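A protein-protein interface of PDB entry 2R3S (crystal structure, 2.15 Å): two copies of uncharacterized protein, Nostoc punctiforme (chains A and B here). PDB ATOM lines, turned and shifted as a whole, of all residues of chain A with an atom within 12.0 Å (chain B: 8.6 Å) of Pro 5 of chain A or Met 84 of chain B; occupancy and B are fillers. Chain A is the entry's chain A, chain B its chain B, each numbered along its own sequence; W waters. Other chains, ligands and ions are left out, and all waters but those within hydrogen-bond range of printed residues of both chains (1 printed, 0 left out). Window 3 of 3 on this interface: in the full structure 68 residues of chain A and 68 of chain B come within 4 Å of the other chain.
Among the printed residues, pairs that only touch across the chains: Pro 5 of chain A with Asp 81 of chain B, Ser 6 of chain A with Phe 85 of chain B, Pro 5 of chain A with Met 84 of chain B, Phe 10 of chain A with Leu 86 of chain B, Pro 7 of chain A with Phe 85 of chain B, Phe 10 of chain A with Gly 95 of chain B, Phe 10 of chain A with Val 94 of chain B and Pro 5 of chain A with Phe 85 of chain B.
Pro 5 of chain A touches just these residues of chain B: Asp 81 (3.0 Å), Met 84 (3.5 Å) and Phe 85 (3.8 Å).
Met 84 of chain B touches one residue of chain A.
Ser 6 of chain A touches just these residues of chain B: Asp 81 and Phe 85.
No residue of chain A comes within 4 Å of Ser 80 of chain B.
Asp 81 of chain B touches just these residues of chain A: Pro 5 (3.0 Å) and Ser 6 (2.9 Å).
Ser 82 of chain B touches none of the printed residues of chain A.
No residue of chain A comes within 4 Å of Ala 83 of chain B.
Of chain A, only Pro 5, Ser 6 and Pro 7 come within 4 Å of Phe 85 of chain B.
No residue of chain A comes within 4 Å of Asp 87 of chain B.
No residue of chain A comes within 4 Å of Ser 90 of chain B.
No residue of chain A comes within 4 Å of Phe 92 of chain B.
Printed residues of chain B within 4 Å of Pro 7 of chain A: Phe 85 (3.6 Å).
Of the printed residues of chain B, Phe 10 of chain A touches Leu 86, Val 94 and Gly 95.
Of the printed residues of chain A, Gly 95 of chain B touches Phe 10.
Of the printed residues of chain A, Val 94 of chain B touches Phe 10.
The nearest residue of chain B that does not touch Pro 5 of chain A is Ser 80 of chain B (5.1 Å).
The nearest printed residue of chain A that does not touch Gly 95 of chain B is Phe 11 of chain A (6.6 Å).
Water W1 lies within hydrogen-bond range of O of Ser 6 of chain A, N of Leu 9 of chain A, N of Ala 8 of chain A and OD2 of Asp 81 of chain B.
The backbone NH of Ala 8 of chain A is in hydrogen-bond range of the side-chain hydroxyl of Ser 6 of chain A.
The backbone carbonyl oxygen (O) of Met 84 of chain B lies within hydrogen-bond range of the side-chain hydroxyl (OG) of Ser 90 of chain B, at 2.5 Å.
The backbone carbonyl oxygen of Phe 85 of chain B is in hydrogen-bond range of the backbone NH of Val 94 of chain B (2.8 Å).
The backbone NH of Ser 6 of chain A lies within hydrogen-bond range of the side-chain carboxylate of Asp 81 of chain B.
No position is printed for both chains.
Of the 9 pairs that touch across the chains among the printed residues, none has its exchanged pair printed and touching as well.
Printed residues of chain B that touch a printed residue of chain A: Asp 81, Met 84, Phe 85, Leu 86, Val 94 and Gly 95.
Of the 9 printed residues of chain A, 4 touch a printed residue of chain B.
Printed residues of chain A that touch a printed residue of chain B: Pro 5, Ser 6, Pro 7 and Phe 10.
Hydrophobic or aromatic side chains of chain A within 4 Å of the printed part of chain B: Pro 5, Pro 7 and Phe 10.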
ATOM      1  N   THR A   4      22.686   4.941  12.173  1.00  0.00           N
ATOM      2  CA  THR A   4      23.892   5.785  11.895  1.00  0.00           C
ATOM      3  C   THR A   4      23.624   6.878  10.834  1.00  0.00           C
ATOM      4  O   THR A   4      22.860   6.661   9.883  1.00  0.00           O
ATOM      5  CB  THR A   4      25.111   4.920  11.455  1.00  0.00           C
ATOM      6  OG1 THR A   4      24.887   4.391  10.138  1.00  0.00           O
ATOM      7  CG2 THR A   4      25.379   3.756  12.469  1.00  0.00           C
ATOM      8  N   PRO A   5      24.266   8.056  10.978  1.00  0.00           N
ATOM      9  CA  PRO A   5      23.934   9.149  10.077  1.00  0.00           C
ATOM     10  C   PRO A   5      24.793   9.083   8.824  1.00  0.00           C
ATOM     11  O   PRO A   5      25.942   8.659   8.895  1.00  0.00           O
ATOM     12  CB  PRO A   5      24.254  10.391  10.913  1.00  0.00           C
ATOM     13  CG  PRO A   5      25.372   9.944  11.813  1.00  0.00           C
ATOM     14  CD  PRO A   5      25.338   8.442  11.914  1.00  0.00           C
ATOM     15  N   SER A   6      24.249   9.519   7.693  1.00  0.00           N
ATOM     16  CA  SER A   6      24.905   9.312   6.420  1.00  0.00           C
ATOM     17  C   SER A   6      24.714  10.432   5.383  1.00  0.00           C
ATOM     18  O   SER A   6      23.608  10.905   5.203  1.00  0.00           O
ATOM     19  CB  SER A   6      24.361   8.035   5.821  1.00  0.00           C
ATOM     20  OG  SER A   6      24.904   7.850   4.547  1.00  0.00           O
ATOM     21  N   PRO A   7      25.786  10.788   4.637  1.00  0.00           N
ATOM     22  CA  PRO A   7      25.702  11.781   3.593  1.00  0.00           C
ATOM     23  C   PRO A   7      25.371  11.156   2.238  1.00  0.00           C
ATOM     24  O   PRO A   7      25.563  11.798   1.212  1.00  0.00           O
ATOM     25  CB  PRO A   7      27.116  12.355   3.576  1.00  0.00           C
ATOM     26  CG  PRO A   7      27.976  11.183   3.871  1.00  0.00           C
ATOM     27  CD  PRO A   7      27.148  10.208   4.683  1.00  0.00           C
ATOM     28  N   ALA A   8      24.863   9.919   2.223  1.00  0.00           N
ATOM     29  CA  ALA A   8      24.567   9.229   0.972  1.00  0.00           C
ATOM     30  C   ALA A   8      23.469   9.909   0.177  1.00  0.00           C
ATOM     31  O   ALA A   8      23.574  10.028  -1.044  1.00  0.00           O
ATOM     32  CB  ALA A   8      24.223   7.744   1.244  1.00  0.00           C
ATOM     33  N   LEU A   9      22.408  10.365   0.841  1.00  0.00           N
ATOM     34  CA  LEU A   9      21.334  11.074   0.127  1.00  0.00           C
ATOM     35  C   LEU A   9      21.885  12.282  -0.600  1.00  0.00           C
ATOM     36  O   LEU A   9      21.609  12.511  -1.791  1.00  0.00           O
ATOM     37  CB  LEU A   9      20.196  11.494   1.082  1.00  0.00           C
ATOM     38  CG  LEU A   9      18.944  12.164   0.462  1.00  0.00           C
ATOM     39  CD1 LEU A   9      18.297  11.338  -0.644  1.00  0.00           C
ATOM     40  CD2 LEU A   9      17.919  12.516   1.538  1.00  0.00           C
ATOM     41  N   PHE A  10      22.647  13.079   0.133  1.00  0.00           N
ATOM     42  CA  PHE A  10      23.282  14.258  -0.439  1.00  0.00           C
ATOM     43  C   PHE A  10      24.048  13.898  -1.714  1.00  0.00           C
ATOM     44  O   PHE A  10      23.831  14.500  -2.743  1.00  0.00           O
ATOM     45  CB  PHE A  10      24.226  14.911   0.554  1.00  0.00           C
ATOM     46  CG  PHE A  10      25.005  16.050  -0.023  1.00  0.00           C
ATOM     47  CD1 PHE A  10      24.355  17.131  -0.597  1.00  0.00           C
ATOM     48  CD2 PHE A  10      26.385  16.061   0.021  1.00  0.00           C
ATOM     49  CE1 PHE A  10      25.063  18.174  -1.126  1.00  0.00           C
ATOM     50  CE2 PHE A  10      27.091  17.117  -0.494  1.00  0.00           C
ATOM     51  CZ  PHE A  10      26.449  18.174  -1.064  1.00  0.00           C
ATOM     52  N   PHE A  11      24.939  12.918  -1.640  1.00  0.00           N
ATOM     53  CA  PHE A  11      25.826  12.619  -2.752  1.00  0.00           C
ATOM     54  C   PHE A  11      25.056  11.962  -3.899  1.00  0.00           C
ATOM     55  O   PHE A  11      25.315  12.260  -5.064  1.00  0.00           O
ATOM     56  CB  PHE A  11      27.040  11.780  -2.310  1.00  0.00           C
ATOM     57  CG  PHE A  11      28.062  12.559  -1.499  1.00  0.00           C
ATOM     58  CD1 PHE A  11      28.744  13.617  -2.050  1.00  0.00           C
ATOM     59  CD2 PHE A  11      28.339  12.223  -0.196  1.00  0.00           C
ATOM     60  CE1 PHE A  11      29.659  14.326  -1.319  1.00  0.00           C
ATOM     61  CE2 PHE A  11      29.261  12.926   0.528  1.00  0.00           C
ATOM     62  CZ  PHE A  11      29.921  13.980  -0.035  1.00  0.00           C
ATOM     63  N   ASN A  12      24.088  11.114  -3.585  1.00  0.00           N
ATOM     64  CA  ASN A  12      23.251  10.528  -4.650  1.00  0.00           C
ATOM     65  C   ASN A  12      22.429  11.579  -5.352  1.00  0.00           C
ATOM     66  O   ASN A  12      22.238  11.512  -6.566  1.00  0.00           O
ATOM     67  CB  ASN A  12      22.329   9.423  -4.104  1.00  0.00           C
ATOM     68  CG  ASN A  12      23.115   8.257  -3.536  1.00  0.00           C
ATOM     69  OD1 ASN A  12      24.238   7.965  -3.978  1.00  0.00           O
ATOM     70  ND2 ASN A  12      22.536   7.587  -2.541  1.00  0.00           N
ATOM     71  N   PHE B  32      20.317  24.903   4.610  1.00  0.00           N
ATOM     72  CA  PHE B  32      20.406  23.948   5.716  1.00  0.00           C
ATOM     73  C   PHE B  32      21.038  24.579   6.930  1.00  0.00           C
ATOM     74  O   PHE B  32      20.703  24.241   8.077  1.00  0.00           O
ATOM     75  CB  PHE B  32      21.176  22.700   5.295  1.00  0.00           C
ATOM     76  CG  PHE B  32      20.653  22.062   4.033  1.00  0.00           C
ATOM     77  CD1 PHE B  32      19.595  21.193   4.073  1.00  0.00           C
ATOM     78  CD2 PHE B  32      21.246  22.321   2.817  1.00  0.00           C
ATOM     79  CE1 PHE B  32      19.096  20.606   2.907  1.00  0.00           C
ATOM     80  CE2 PHE B  32      20.770  21.732   1.657  1.00  0.00           C
ATOM     81  CZ  PHE B  32      19.690  20.867   1.715  1.00  0.00           C
ATOM     82  N   SER B  36      19.231  24.821  10.467  1.00  0.00           N
ATOM     83  CA  SER B  36      20.072  24.238  11.522  1.00  0.00           C
ATOM     84  C   SER B  36      19.288  23.150  12.281  1.00  0.00           C
ATOM     85  O   SER B  36      18.613  22.337  11.642  1.00  0.00           O
ATOM     86  CB  SER B  36      20.650  25.327  12.443  1.00  0.00           C
ATOM     87  OG  SER B  36      21.799  24.836  13.158  1.00  0.00           O
ATOM     88  N   GLN B  37      19.377  23.109  13.617  1.00  0.00           N
ATOM     89  CA  GLN B  37      18.594  22.138  14.408  1.00  0.00           C
ATOM     90  C   GLN B  37      17.256  22.704  14.915  1.00  0.00           C
ATOM     91  O   GLN B  37      16.624  22.119  15.790  1.00  0.00           O
ATOM     92  CB  GLN B  37      19.443  21.556  15.553  1.00  0.00           C
ATOM     93  CG  GLN B  37      20.790  21.057  15.045  1.00  0.00           C
ATOM     94  CD  GLN B  37      21.517  20.108  15.966  1.00  0.00           C
ATOM     95  OE1 GLN B  37      21.040  19.746  17.043  1.00  0.00           O
ATOM     96  NE2 GLN B  37      22.694  19.682  15.528  1.00  0.00           N
ATOM     97  N   LEU B  78      15.322  20.006   9.715  1.00  0.00           N
ATOM     98  CA  LEU B  78      16.277  19.108   9.084  1.00  0.00           C
ATOM     99  C   LEU B  78      16.107  17.656   9.564  1.00  0.00           C
ATOM    100  O   LEU B  78      15.667  17.395  10.671  1.00  0.00           O
ATOM    101  CB  LEU B  78      17.736  19.590   9.306  1.00  0.00           C
ATOM    102  CG  LEU B  78      18.106  20.930   8.642  1.00  0.00           C
ATOM    103  CD1 LEU B  78      19.614  21.201   8.759  1.00  0.00           C
ATOM    104  CD2 LEU B  78      17.659  21.010   7.189  1.00  0.00           C
ATOM    105  N   THR B  79      16.410  16.708   8.681  1.00  0.00           N
ATOM    106  CA  THR B  79      16.732  15.356   9.106  1.00  0.00           C
ATOM    107  C   THR B  79      18.096  15.398   9.805  1.00  0.00           C
ATOM    108  O   THR B  79      18.867  16.371   9.701  1.00  0.00           O
ATOM    109  CB  THR B  79      16.795  14.384   7.914  1.00  0.00           C
ATOM    110  OG1 THR B  79      17.862  14.765   7.049  1.00  0.00           O
ATOM    111  CG2 THR B  79      15.483  14.366   7.133  1.00  0.00           C
ATOM    112  N   SER B  80      18.381  14.347  10.551  1.00  0.00           N
ATOM    113  CA  SER B  80      19.637  14.218  11.248  1.00  0.00           C
ATOM    114  C   SER B  80      20.799  14.289  10.319  1.00  0.00           C
ATOM    115  O   SER B  80      21.838  14.844  10.663  1.00  0.00           O
ATOM    116  CB  SER B  80      19.706  12.850  11.915  1.00  0.00           C
ATOM    117  OG  SER B  80      18.896  12.893  13.039  1.00  0.00           O
ATOM    118  N   ASP B  81      20.644  13.639   9.177  1.00  0.00           N
ATOM    119  CA  ASP B  81      21.674  13.590   8.144  1.00  0.00           C
ATOM    120  C   ASP B  81      21.991  14.967   7.579  1.00  0.00           C
ATOM    121  O   ASP B  81      23.171  15.312   7.407  1.00  0.00           O
ATOM    122  CB  ASP B  81      21.265  12.599   7.049  1.00  0.00           C
ATOM    123  CG  ASP B  81      21.246  11.157   7.566  1.00  0.00           C
ATOM    124  OD1 ASP B  81      21.905  10.883   8.602  1.00  0.00           O
ATOM    125  OD2 ASP B  81      20.601  10.287   6.967  1.00  0.00           O
ATOM    126  N   SER B  82      20.951  15.769   7.349  1.00  0.00           N
ATOM    127  CA  SER B  82      21.138  17.144   6.872  1.00  0.00           C
ATOM    128  C   SER B  82      21.759  18.041   7.951  1.00  0.00           C
ATOM    129  O   SER B  82      22.645  18.830   7.672  1.00  0.00           O
ATOM    130  CB  SER B  82      19.811  17.726   6.349  1.00  0.00           C
ATOM    131  OG  SER B  82      19.424  17.109   5.121  1.00  0.00           O
ATOM    132  N   ALA B  83      21.289  17.914   9.188  1.00  0.00           N
ATOM    133  CA  ALA B  83      21.884  18.605  10.334  1.00  0.00           C
ATOM    134  C   ALA B  83      23.384  18.291  10.470  1.00  0.00           C
ATOM    135  O   ALA B  83      24.203  19.161  10.783  1.00  0.00           O
ATOM    136  CB  ALA B  83      21.152  18.180  11.645  1.00  0.00           C
ATOM    137  N   MET B  84      23.729  17.033  10.247  1.00  0.00           N
ATOM    138  CA  MET B  84      25.102  16.589  10.365  1.00  0.00           C
ATOM    139  C   MET B  84      26.030  17.060   9.237  1.00  0.00           C
ATOM    140  O   MET B  84      27.117  17.543   9.513  1.00  0.00           O
ATOM    141  CB  MET B  84      25.117  15.080  10.413  1.00  0.00           C
ATOM    142  CG  MET B  84      26.510  14.488  10.460  1.00  0.00           C
ATOM    143  SD  MET B  84      26.606  13.225  11.933  1.00  0.00           S
ATOM    144  CE  MET B  84      26.302  14.657  13.265  1.00  0.00           C
ATOM    145  N   PHE B  85      25.585  16.911   7.984  1.00  0.00           N
ATOM    146  CA  PHE B  85      26.423  17.047   6.791  1.00  0.00           C
ATOM    147  C   PHE B  85      26.224  18.297   5.941  1.00  0.00           C
ATOM    148  O   PHE B  85      27.063  18.598   5.079  1.00  0.00           O
ATOM    149  CB  PHE B  85      26.239  15.792   5.901  1.00  0.00           C
ATOM    150  CG  PHE B  85      26.704  14.543   6.573  1.00  0.00           C
ATOM    151  CD1 PHE B  85      28.073  14.323   6.775  1.00  0.00           C
ATOM    152  CD2 PHE B  85      25.801  13.613   7.070  1.00  0.00           C
ATOM    153  CE1 PHE B  85      28.537  13.175   7.462  1.00  0.00           C
ATOM    154  CE2 PHE B  85      26.259  12.473   7.755  1.00  0.00           C
ATOM    155  CZ  PHE B  85      27.629  12.261   7.947  1.00  0.00           C
ATOM    156  N   LEU B  86      25.122  19.010   6.152  1.00  0.00           N
ATOM    157  CA  LEU B  86      24.756  20.130   5.287  1.00  0.00           C
ATOM    158  C   LEU B  86      24.583  21.449   6.019  1.00  0.00           C
ATOM    159  O   LEU B  86      24.438  22.490   5.376  1.00  0.00           O
ATOM    160  CB  LEU B  86      23.476  19.791   4.497  1.00  0.00           C
ATOM    161  CG  LEU B  86      23.647  18.611   3.532  1.00  0.00           C
ATOM    162  CD1 LEU B  86      22.339  18.125   2.965  1.00  0.00           C
ATOM    163  CD2 LEU B  86      24.597  19.029   2.417  1.00  0.00           C
ATOM    164  N   ASP B  87      24.607  21.413   7.337  1.00  0.00           N
ATOM    165  CA  ASP B  87      24.562  22.640   8.168  1.00  0.00           C
ATOM    166  C   ASP B  87      26.001  23.051   8.377  1.00  0.00           C
ATOM    167  O   ASP B  87      26.784  22.271   8.900  1.00  0.00           O
ATOM    168  CB  ASP B  87      23.910  22.328   9.502  1.00  0.00           C
ATOM    169  CG  ASP B  87      23.898  23.510  10.485  1.00  0.00           C
ATOM    170  OD1 ASP B  87      24.421  24.600  10.206  1.00  0.00           O
ATOM    171  OD2 ASP B  87      23.346  23.313  11.580  1.00  0.00           O
ATOM    172  N   ARG B  88      26.382  24.252   7.944  1.00  0.00           N
ATOM    173  CA  ARG B  88      27.798  24.668   8.060  1.00  0.00           C
ATOM    174  C   ARG B  88      28.337  24.681   9.494  1.00  0.00           C
ATOM    175  O   ARG B  88      29.557  24.637   9.707  1.00  0.00           O
ATOM    176  CB  ARG B  88      28.011  26.028   7.436  1.00  0.00           C
ATOM    177  CG  ARG B  88      27.817  26.038   5.921  1.00  0.00           C
ATOM    178  CD  ARG B  88      28.108  27.445   5.384  1.00  0.00           C
ATOM    179  NE  ARG B  88      27.878  27.506   3.950  1.00  0.00           N
ATOM    180  CZ  ARG B  88      28.751  27.121   3.015  1.00  0.00           C
ATOM    181  NH1 ARG B  88      29.941  26.644   3.337  1.00  0.00           N
ATOM    182  NH2 ARG B  88      28.420  27.229   1.733  1.00  0.00           N
ATOM    183  N   GLN B  89      27.428  24.751  10.462  1.00  0.00           N
ATOM    184  CA  GLN B  89      27.781  24.798  11.866  1.00  0.00           C
ATOM    185  C   GLN B  89      28.301  23.441  12.321  1.00  0.00           C
ATOM    186  O   GLN B  89      28.979  23.349  13.355  1.00  0.00           O
ATOM    187  CB  GLN B  89      26.536  25.179  12.660  1.00  0.00           C
ATOM    188  CG  GLN B  89      26.657  25.230  14.181  1.00  0.00           C
ATOM    189  CD  GLN B  89      25.295  25.019  14.868  1.00  0.00           C
ATOM    190  OE1 GLN B  89      24.661  25.984  15.324  1.00  0.00           O
ATOM    191  NE2 GLN B  89      24.835  23.752  14.925  1.00  0.00           N
ATOM    192  N   SER B  90      27.999  22.388  11.566  1.00  0.00           N
ATOM    193  CA  SER B  90      28.464  21.053  11.920  1.00  0.00           C
ATOM    194  C   SER B  90      29.890  20.813  11.461  1.00  0.00           C
ATOM    195  O   SER B  90      30.250  21.172  10.341  1.00  0.00           O
ATOM    196  CB  SER B  90      27.553  20.009  11.284  1.00  0.00           C
ATOM    197  OG  SER B  90      28.053  18.716  11.505  1.00  0.00           O
ATOM    198  N   LYS B  91      30.680  20.187  12.333  1.00  0.00           N
ATOM    199  CA  LYS B  91      32.066  19.808  12.070  1.00  0.00           C
ATOM    200  C   LYS B  91      32.197  18.876  10.884  1.00  0.00           C
ATOM    201  O   LYS B  91      33.278  18.733  10.343  1.00  0.00           O
ATOM    202  CB  LYS B  91      32.691  19.127  13.317  1.00  0.00           C
ATOM    203  N   PHE B  92      31.099  18.246  10.480  1.00  0.00           N
ATOM    204  CA  PHE B  92      31.100  17.244   9.432  1.00  0.00           C
ATOM    205  C   PHE B  92      30.486  17.752   8.147  1.00  0.00           C
ATOM    206  O   PHE B  92      30.155  16.956   7.286  1.00  0.00           O
ATOM    207  CB  PHE B  92      30.313  15.999   9.880  1.00  0.00           C
ATOM    208  CG  PHE B  92      30.775  15.420  11.186  1.00  0.00           C
ATOM    209  CD1 PHE B  92      31.865  14.556  11.231  1.00  0.00           C
ATOM    210  CD2 PHE B  92      30.112  15.736  12.375  1.00  0.00           C
ATOM    211  CE1 PHE B  92      32.295  14.017  12.436  1.00  0.00           C
ATOM    212  CE2 PHE B  92      30.529  15.205  13.592  1.00  0.00           C
ATOM    213  CZ  PHE B  92      31.622  14.337  13.624  1.00  0.00           C
ATOM    214  N   TYR B  93      30.336  19.060   8.016  1.00  0.00           N
ATOM    215  CA  TYR B  93      29.764  19.669   6.806  1.00  0.00           C
ATOM    216  C   TYR B  93      30.542  19.316   5.526  1.00  0.00           C
ATOM    217  O   TYR B  93      31.744  19.518   5.448  1.00  0.00           O
ATOM    218  CB  TYR B  93      29.699  21.192   6.973  1.00  0.00           C
ATOM    219  CG  TYR B  93      29.295  21.924   5.729  1.00  0.00           C
ATOM    220  CD1 TYR B  93      27.968  22.023   5.373  1.00  0.00           C
ATOM    221  CD2 TYR B  93      30.242  22.518   4.901  1.00  0.00           C
ATOM    222  CE1 TYR B  93      27.587  22.662   4.233  1.00  0.00           C
ATOM    223  CE2 TYR B  93      29.855  23.168   3.742  1.00  0.00           C
ATOM    224  CZ  TYR B  93      28.521  23.244   3.425  1.00  0.00           C
ATOM    225  OH  TYR B  93      28.094  23.895   2.282  1.00  0.00           O
ATOM    226  N   VAL B  94      29.831  18.809   4.522  1.00  0.00           N
ATOM    227  CA  VAL B  94      30.434  18.355   3.295  1.00  0.00           C
ATOM    228  C   VAL B  94      29.800  19.071   2.116  1.00  0.00           C
ATOM    229  O   VAL B  94      30.098  18.776   0.976  1.00  0.00           O
ATOM    230  CB  VAL B  94      30.291  16.796   3.122  1.00  0.00           C
ATOM    231  CG1 VAL B  94      31.195  16.033   4.124  1.00  0.00           C
ATOM    232  CG2 VAL B  94      28.828  16.356   3.262  1.00  0.00           C
ATOM    233  N   GLY B  95      28.931  20.037   2.370  1.00  0.00           N
ATOM    234  CA  GLY B  95      28.140  20.627   1.281  1.00  0.00           C
ATOM    235  C   GLY B  95      28.961  21.235   0.168  1.00  0.00           C
ATOM    236  O   GLY B  95      28.552  21.237  -0.987  1.00  0.00           O
HETATM  237  O   HOH W   1      21.766   9.829   3.741  1.00  0.00           O
